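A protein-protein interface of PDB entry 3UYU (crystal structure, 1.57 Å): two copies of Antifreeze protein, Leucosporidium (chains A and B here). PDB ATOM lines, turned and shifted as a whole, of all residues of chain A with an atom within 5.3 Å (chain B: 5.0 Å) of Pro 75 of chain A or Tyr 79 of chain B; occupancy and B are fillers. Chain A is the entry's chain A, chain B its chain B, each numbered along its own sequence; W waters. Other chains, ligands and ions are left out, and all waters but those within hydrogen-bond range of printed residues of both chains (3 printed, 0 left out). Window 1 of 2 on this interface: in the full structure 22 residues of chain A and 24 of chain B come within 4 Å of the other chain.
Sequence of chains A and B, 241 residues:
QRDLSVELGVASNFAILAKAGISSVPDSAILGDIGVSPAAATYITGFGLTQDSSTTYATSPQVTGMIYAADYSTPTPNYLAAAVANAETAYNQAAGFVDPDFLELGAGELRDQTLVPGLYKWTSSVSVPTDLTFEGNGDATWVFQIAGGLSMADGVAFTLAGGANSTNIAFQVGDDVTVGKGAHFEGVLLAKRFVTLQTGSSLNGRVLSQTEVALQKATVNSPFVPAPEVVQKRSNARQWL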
ATOM      1  N   SER A  73      -1.321  -1.985 -20.269  1.00  0.00           N
ATOM      2  CA  SER A  73       0.122  -1.989 -20.002  1.00  0.00           C
ATOM      3  C   SER A  73       0.821  -0.841 -20.670  1.00  0.00           C
ATOM      4  O   SER A  73       0.434  -0.379 -21.731  1.00  0.00           O
ATOM      5  CB  SER A  73       0.687  -3.300 -20.553  1.00  0.00           C
ATOM      6  OG  SER A  73       0.025  -4.394 -19.908  1.00  0.00           O
ATOM      7  N   THR A  74       1.937  -0.468 -20.061  1.00  0.00           N
ATOM      8  CA  THR A  74       2.895   0.488 -20.635  1.00  0.00           C
ATOM      9  C   THR A  74       3.277   0.214 -22.096  1.00  0.00           C
ATOM     10  O   THR A  74       3.614  -0.938 -22.472  1.00  0.00           O
ATOM     11  CB  THR A  74       4.156   0.483 -19.656  1.00  0.00           C
ATOM     12  OG1 THR A  74       3.692   0.695 -18.294  1.00  0.00           O
ATOM     13  CG2 THR A  74       5.047   1.586 -19.984  1.00  0.00           C
ATOM     14  N   PRO A  75       3.292   1.255 -22.961  1.00  0.00           N
ATOM     15  CA  PRO A  75       3.133   2.705 -22.689  1.00  0.00           C
ATOM     16  C   PRO A  75       1.698   3.224 -22.827  1.00  0.00           C
ATOM     17  O   PRO A  75       1.492   4.441 -22.940  1.00  0.00           O
ATOM     18  CB  PRO A  75       3.946   3.333 -23.813  1.00  0.00           C
ATOM     19  CG  PRO A  75       3.837   2.405 -24.920  1.00  0.00           C
ATOM     20  CD  PRO A  75       3.684   1.040 -24.370  1.00  0.00           C
ATOM     21  N   THR A  76       0.695   2.323 -22.793  1.00  0.00           N
ATOM     22  CA  THR A  76      -0.647   2.854 -23.043  1.00  0.00           C
ATOM     23  C   THR A  76      -1.164   3.914 -22.063  1.00  0.00           C
ATOM     24  O   THR A  76      -1.751   4.930 -22.495  1.00  0.00           O
ATOM     25  CB  THR A  76      -1.618   1.682 -23.246  1.00  0.00           C
ATOM     26  OG1 THR A  76      -1.232   0.980 -24.416  1.00  0.00           O
ATOM     27  CG2 THR A  76      -3.127   2.122 -23.337  1.00  0.00           C
ATOM     28  N   PRO A  77      -0.945   3.771 -20.720  1.00  0.00           N
ATOM     29  CA  PRO A  77      -1.402   4.830 -19.835  1.00  0.00           C
ATOM     30  C   PRO A  77      -0.819   6.239 -20.164  1.00  0.00           C
ATOM     31  O   PRO A  77      -1.559   7.199 -20.168  1.00  0.00           O
ATOM     32  CB  PRO A  77      -1.033   4.285 -18.393  1.00  0.00           C
ATOM     33  CG  PRO A  77      -1.028   2.766 -18.616  1.00  0.00           C
ATOM     34  CD  PRO A  77      -0.435   2.592 -19.967  1.00  0.00           C
ATOM     35  N   ASN A  78       0.485   6.300 -20.472  1.00  0.00           N
ATOM     36  CA  ASN A  78       1.055   7.618 -20.722  1.00  0.00           C
ATOM     37  C   ASN A  78       0.693   8.150 -22.127  1.00  0.00           C
ATOM     38  O   ASN A  78       0.584   9.346 -22.266  1.00  0.00           O
ATOM     39  CB  ASN A  78       2.590   7.600 -20.512  1.00  0.00           C
ATOM     40  CG  ASN A  78       2.946   7.626 -19.036  1.00  0.00           C
ATOM     41  OD1 ASN A  78       2.235   8.160 -18.223  1.00  0.00           O
ATOM     42  ND2 ASN A  78       4.086   7.107 -18.744  1.00  0.00           N
ATOM     43  N   TYR A  79       0.476   7.237 -23.099  1.00  0.00           N
ATOM     44  CA  TYR A  79      -0.020   7.626 -24.434  1.00  0.00           C
ATOM     45  C   TYR A  79      -1.428   8.244 -24.320  1.00  0.00           C
ATOM     46  O   TYR A  79      -1.686   9.334 -24.855  1.00  0.00           O
ATOM     47  CB  TYR A  79      -0.055   6.378 -25.278  1.00  0.00           C
ATOM     48  CG  TYR A  79      -0.542   6.571 -26.716  1.00  0.00           C
ATOM     49  CD1 TYR A  79       0.135   7.424 -27.614  1.00  0.00           C
ATOM     50  CD2 TYR A  79      -1.659   5.859 -27.144  1.00  0.00           C
ATOM     51  CE1 TYR A  79      -0.316   7.562 -28.937  1.00  0.00           C
ATOM     52  CE2 TYR A  79      -2.081   5.960 -28.490  1.00  0.00           C
ATOM     53  CZ  TYR A  79      -1.417   6.820 -29.349  1.00  0.00           C
ATOM     54  OH  TYR A  79      -1.810   7.001 -30.685  1.00  0.00           O
ATOM     55  N   LEU A  80      -2.303   7.556 -23.593  1.00  0.00           N
ATOM     56  CA  LEU A  80      -3.626   8.086 -23.320  1.00  0.00           C
ATOM     57  C   LEU A  80      -3.670   9.387 -22.529  1.00  0.00           C
ATOM     58  O   LEU A  80      -4.502  10.304 -22.776  1.00  0.00           O
ATOM     59  CB  LEU A  80      -4.497   7.016 -22.595  1.00  0.00           C
ATOM     60  CG  LEU A  80      -5.044   5.872 -23.484  1.00  0.00           C
ATOM     61  CD1 LEU A  80      -5.517   4.790 -22.537  1.00  0.00           C
ATOM     62  CD2 LEU A  80      -6.195   6.409 -24.373  1.00  0.00           C
ATOM     63  N   VAL B  10       5.022  15.361 -23.726  1.00  0.00           N
ATOM     64  CA  VAL B  10       5.368  13.978 -23.517  1.00  0.00           C
ATOM     65  C   VAL B  10       6.870  13.782 -23.196  1.00  0.00           C
ATOM     66  O   VAL B  10       7.254  12.735 -22.663  1.00  0.00           O
ATOM     67  CB  VAL B  10       4.933  13.154 -24.801  1.00  0.00           C
ATOM     68  CG1 VAL B  10       5.281  11.708 -24.688  1.00  0.00           C
ATOM     69  CG2 VAL B  10       3.470  13.314 -25.046  1.00  0.00           C
ATOM     70  N   ASN B  13       8.170  12.487 -19.899  1.00  0.00           N
ATOM     71  CA  ASN B  13       8.221  11.046 -19.574  1.00  0.00           C
ATOM     72  C   ASN B  13       9.571  10.404 -19.913  1.00  0.00           C
ATOM     73  O   ASN B  13       9.695   9.171 -19.776  1.00  0.00           O
ATOM     74  CB  ASN B  13       7.101  10.359 -20.374  1.00  0.00           C
ATOM     75  CG  ASN B  13       5.762  10.973 -20.126  1.00  0.00           C
ATOM     76  OD1 ASN B  13       5.573  11.807 -19.223  1.00  0.00           O
ATOM     77  ND2 ASN B  13       4.851  10.710 -21.014  1.00  0.00           N
ATOM     78  N   PHE B  14      10.629  11.183 -20.287  1.00  0.00           N
ATOM     79  CA  PHE B  14      11.915  10.597 -20.697  1.00  0.00           C
ATOM     80  C   PHE B  14      13.054  11.194 -19.957  1.00  0.00           C
ATOM     81  O   PHE B  14      13.164  12.447 -19.802  1.00  0.00           O
ATOM     82  CB  PHE B  14      12.090  10.793 -22.223  1.00  0.00           C
ATOM     83  CG  PHE B  14      11.200   9.909 -23.018  1.00  0.00           C
ATOM     84  CD1 PHE B  14       9.928  10.323 -23.368  1.00  0.00           C
ATOM     85  CD2 PHE B  14      11.686   8.684 -23.468  1.00  0.00           C
ATOM     86  CE1 PHE B  14       9.101   9.450 -24.108  1.00  0.00           C
ATOM     87  CE2 PHE B  14      10.868   7.833 -24.235  1.00  0.00           C
ATOM     88  CZ  PHE B  14       9.589   8.232 -24.531  1.00  0.00           C
ATOM     89  N   ASP B  33      12.713   6.666 -18.346  1.00  0.00           N
ATOM     90  CA  ASP B  33      12.639   5.964 -19.638  1.00  0.00           C
ATOM     91  C   ASP B  33      13.632   6.542 -20.651  1.00  0.00           C
ATOM     92  O   ASP B  33      14.024   7.731 -20.566  1.00  0.00           O
ATOM     93  CB  ASP B  33      11.216   6.075 -20.236  1.00  0.00           C
ATOM     94  CG  ASP B  33      10.173   5.419 -19.350  1.00  0.00           C
ATOM     95  OD1 ASP B  33      10.517   4.525 -18.558  1.00  0.00           O
ATOM     96  OD2 ASP B  33       8.944   5.762 -19.543  1.00  0.00           O
ATOM     97  N   THR B  56       6.624  -4.032 -27.395  1.00  0.00           N
ATOM     98  CA  THR B  56       6.398  -2.577 -27.351  1.00  0.00           C
ATOM     99  C   THR B  56       7.573  -1.854 -26.683  1.00  0.00           C
ATOM    100  O   THR B  56       7.738  -0.646 -26.862  1.00  0.00           O
ATOM    101  CB  THR B  56       5.118  -2.165 -26.575  1.00  0.00           C
ATOM    102  OG1 THR B  56       5.158  -2.724 -25.260  1.00  0.00           O
ATOM    103  CG2 THR B  56       3.859  -2.624 -27.303  1.00  0.00           C
ATOM    104  N   TYR B  68      12.384   2.511 -25.428  1.00  0.00           N
ATOM    105  CA  TYR B  68      11.441   2.517 -26.585  1.00  0.00           C
ATOM    106  C   TYR B  68      12.218   2.872 -27.820  1.00  0.00           C
ATOM    107  O   TYR B  68      13.125   3.766 -27.811  1.00  0.00           O
ATOM    108  CB  TYR B  68      10.344   3.633 -26.350  1.00  0.00           C
ATOM    109  CG  TYR B  68       9.413   3.368 -25.163  1.00  0.00           C
ATOM    110  CD1 TYR B  68       8.402   2.450 -25.238  1.00  0.00           C
ATOM    111  CD2 TYR B  68       9.573   4.063 -23.952  1.00  0.00           C
ATOM    112  CE1 TYR B  68       7.620   2.154 -24.172  1.00  0.00           C
ATOM    113  CE2 TYR B  68       8.776   3.813 -22.865  1.00  0.00           C
ATOM    114  CZ  TYR B  68       7.768   2.841 -22.998  1.00  0.00           C
ATOM    115  OH  TYR B  68       6.939   2.537 -21.941  1.00  0.00           O
ATOM    116  N   PRO B  75       1.380   0.848 -29.236  1.00  0.00           N
ATOM    117  CA  PRO B  75       1.378   2.260 -29.729  1.00  0.00           C
ATOM    118  C   PRO B  75       2.752   2.971 -29.606  1.00  0.00           C
ATOM    119  O   PRO B  75       2.782   4.198 -29.634  1.00  0.00           O
ATOM    120  CB  PRO B  75       0.369   2.939 -28.808  1.00  0.00           C
ATOM    121  CG  PRO B  75       0.663   2.252 -27.447  1.00  0.00           C
ATOM    122  CD  PRO B  75       0.955   0.806 -27.815  1.00  0.00           C
ATOM    123  N   THR B  76       3.823   2.205 -29.533  1.00  0.00           N
ATOM    124  CA  THR B  76       5.171   2.860 -29.303  1.00  0.00           C
ATOM    125  C   THR B  76       5.554   3.833 -30.420  1.00  0.00           C
ATOM    126  O   THR B  76       6.015   4.922 -30.105  1.00  0.00           O
ATOM    127  CB  THR B  76       6.194   1.829 -28.999  1.00  0.00           C
ATOM    128  OG1 THR B  76       5.866   1.259 -27.710  1.00  0.00           O
ATOM    129  CG2 THR B  76       7.626   2.485 -28.941  1.00  0.00           C
ATOM    130  N   PRO B  77       5.332   3.485 -31.717  1.00  0.00           N
ATOM    131  CA  PRO B  77       5.712   4.479 -32.749  1.00  0.00           C
ATOM    132  C   PRO B  77       5.004   5.837 -32.576  1.00  0.00           C
ATOM    133  O   PRO B  77       5.685   6.903 -32.619  1.00  0.00           O
ATOM    134  CB  PRO B  77       5.269   3.771 -34.053  1.00  0.00           C
ATOM    135  CG  PRO B  77       5.635   2.318 -33.707  1.00  0.00           C
ATOM    136  CD  PRO B  77       5.059   2.138 -32.329  1.00  0.00           C
ATOM    137  N   ASN B  78       3.702   5.848 -32.326  1.00  0.00           N
ATOM    138  CA  ASN B  78       2.973   7.116 -32.210  1.00  0.00           C
ATOM    139  C   ASN B  78       3.317   7.812 -30.868  1.00  0.00           C
ATOM    140  O   ASN B  78       3.315   9.028 -30.829  1.00  0.00           O
ATOM    141  CB  ASN B  78       1.440   6.881 -32.209  1.00  0.00           C
ATOM    142  CG  ASN B  78       0.900   6.592 -33.558  1.00  0.00           C
ATOM    143  OD1 ASN B  78       1.528   6.888 -34.556  1.00  0.00           O
ATOM    144  ND2 ASN B  78      -0.313   6.041 -33.588  1.00  0.00           N
ATOM    145  N   TYR B  79       3.586   7.015 -29.840  1.00  0.00           N
ATOM    146  CA  TYR B  79       3.943   7.587 -28.521  1.00  0.00           C
ATOM    147  C   TYR B  79       5.283   8.347 -28.715  1.00  0.00           C
ATOM    148  O   TYR B  79       5.409   9.498 -28.247  1.00  0.00           O
ATOM    149  CB  TYR B  79       4.024   6.422 -27.520  1.00  0.00           C
ATOM    150  CG  TYR B  79       4.540   6.818 -26.151  1.00  0.00           C
ATOM    151  CD1 TYR B  79       3.802   7.711 -25.323  1.00  0.00           C
ATOM    152  CD2 TYR B  79       5.747   6.301 -25.676  1.00  0.00           C
ATOM    153  CE1 TYR B  79       4.249   8.072 -24.034  1.00  0.00           C
ATOM    154  CE2 TYR B  79       6.188   6.652 -24.363  1.00  0.00           C
ATOM    155  CZ  TYR B  79       5.430   7.547 -23.603  1.00  0.00           C
ATOM    156  OH  TYR B  79       5.775   7.905 -22.310  1.00  0.00           O
ATOM    157  N   LEU B  80       6.265   7.680 -29.294  1.00  0.00           N
ATOM    158  CA  LEU B  80       7.568   8.354 -29.590  1.00  0.00           C
ATOM    159  C   LEU B  80       7.443   9.530 -30.536  1.00  0.00           C
ATOM    160  O   LEU B  80       8.181  10.539 -30.364  1.00  0.00           O
ATOM    161  CB  LEU B  80       8.653   7.379 -30.071  1.00  0.00           C
ATOM    162  CG  LEU B  80       9.183   6.326 -29.126  1.00  0.00           C
ATOM    163  CD1 LEU B  80       9.846   5.253 -29.969  1.00  0.00           C
ATOM    164  CD2 LEU B  80      10.166   7.030 -28.163  1.00  0.00           C
ATOM    165  N   ALA B  81       6.588   9.402 -31.578  1.00  0.00           N
ATOM    166  CA  ALA B  81       6.504  10.544 -32.501  1.00  0.00           C
ATOM    167  C   ALA B  81       5.996  11.793 -31.734  1.00  0.00           C
ATOM    168  O   ALA B  81       6.472  12.921 -31.928  1.00  0.00           O
ATOM    169  CB  ALA B  81       5.503  10.158 -33.666  1.00  0.00           C
ATOM    170  N   ALA B  82       5.076  11.612 -30.790  1.00  0.00           N
ATOM    171  CA  ALA B  82       4.612  12.706 -29.906  1.00  0.00           C
ATOM    172  C   ALA B  82       5.731  13.228 -29.004  1.00  0.00           C
ATOM    173  O   ALA B  82       5.891  14.414 -28.821  1.00  0.00           O
ATOM    174  CB  ALA B  82       3.453  12.177 -29.013  1.00  0.00           C
ATOM    175  N   ALA B  83       6.472  12.298 -28.389  1.00  0.00           N
ATOM    176  CA  ALA B  83       7.576  12.748 -27.524  1.00  0.00           C
ATOM    177  C   ALA B  83       8.628  13.613 -28.292  1.00  0.00           C
ATOM    178  O   ALA B  83       9.050  14.676 -27.793  1.00  0.00           O
ATOM    179  CB  ALA B  83       8.271  11.495 -26.964  1.00  0.00           C
HETATM  180  O   HOH W   1       7.052   7.216 -18.115  1.00  0.00           O
HETATM  181  O   HOH W   2       1.960  11.238 -20.798  1.00  0.00           O
HETATM  182  O   HOH W   3      -0.832   4.082 -31.707  1.00  0.00           O
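Hydrophobic or aromatic side chains of chain B that line the printed part of chain A: Tyr 68, Pro 75 and Tyr 79.
The backbone carbonyl oxygen (O) of Ser 73 of chain A sits close to the side-chain hydroxyl (OG1) of Thr 76 of chain A (3.4 Å).
The side-chain amide nitrogen of Asn 13 of chain B is in hydrogen-bond range of the side-chain hydroxyl of Tyr 79 of chain B (3.2 Å).
The backbone carbonyl oxygen of Thr 56 of chain B sits at hydrogen-bond distance from the side-chain hydroxyl of Thr 76 of chain B (2.8 Å).
Pro 75 of chain A touches three residues of chain B.
Printed residues of chain A within 4 Å of Tyr 79 of chain B: Pro 75, Asn 78 and Tyr 79.
Of the printed residues of chain A, Thr 56 of chain B touches Thr 74 (3.7 Å).
Printed residues of chain A within 4 Å of Thr 76 of chain B: Pro 75.
Printed residues of chain A within 4 Å of Pro 75 of chain B: Thr 76 and Tyr 79.
Of the printed residues of chain A, Asn 13 of chain B touches Asn 78.
Pro 77 of chain A touches none of the printed residues of chain B.
Among the printed residues, merely in contact across the chains: Thr 74 of chain A with Tyr 68 of chain B (2.9 Å), Pro 75 of chain A with Tyr 68 of chain B (3.6 Å), Pro 75 of chain A with Thr 76 of chain B (3.6 Å), Thr 74 of chain A with Thr 56 of chain B (3.7 Å), Asn 78 of chain A with Tyr 79 of chain B (3.7 Å), Thr 76 of chain A with Pro 75 of chain B (3.8 Å), Asn 78 of chain A with Asn 13 of chain B (3.9 Å), Tyr 79 of chain A with Pro 75 of chain B (3.9 Å), Tyr 79 of chain A with Tyr 79 of chain B (3.9 Å) and Pro 75 of chain A with Tyr 79 of chain B (3.9 Å).
Water W2 lies within hydrogen-bond range of the backbone carbonyl oxygen of Asn 78 of chain A (2.8 Å) and the side-chain amide nitrogen of Asn 13 of chain B (2.9 Å).
Water W3 bridges the side-chain amide nitrogen (ND2) of Asn 78 of chain B (2.8 Å) and the side-chain hydroxyl (OH) of Tyr 79 of chain A (3.2 Å).
Water W1 lies within hydrogen-bond range of the side-chain carboxylate of Asp 33 of chain B (2.8 Å) and the side-chain amide nitrogen of Asn 78 of chain A (3.0 Å).
Pro 75 of chain A touches Thr 76 of chain B, and with the chains exchanged Thr 76 of chain A touches Pro 75 of chain B.
Pro 75 of chain A touches Tyr 79 of chain B, and with the chains exchanged Tyr 79 of chain A touches Pro 75 of chain B.
Asn 78 of chain A touches Tyr 79 of chain B, and with the chains exchanged Tyr 79 of chain A touches Asn 78 of chain B.
Tyr 79 of chain A touches its own counterpart, Tyr 79 of chain B.
Positions printed for both chains: 75, 76, 77, 78, 79 and 80.
Of the 11 pairs that touch across the chains among the printed residues, 7 have their exchanged pair printed and touching as well.
The side-chain hydroxyl (OH) of Tyr 79 of chain A lies within hydrogen-bond range of the side-chain amide nitrogen (ND2) of Asn 78 of chain B.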
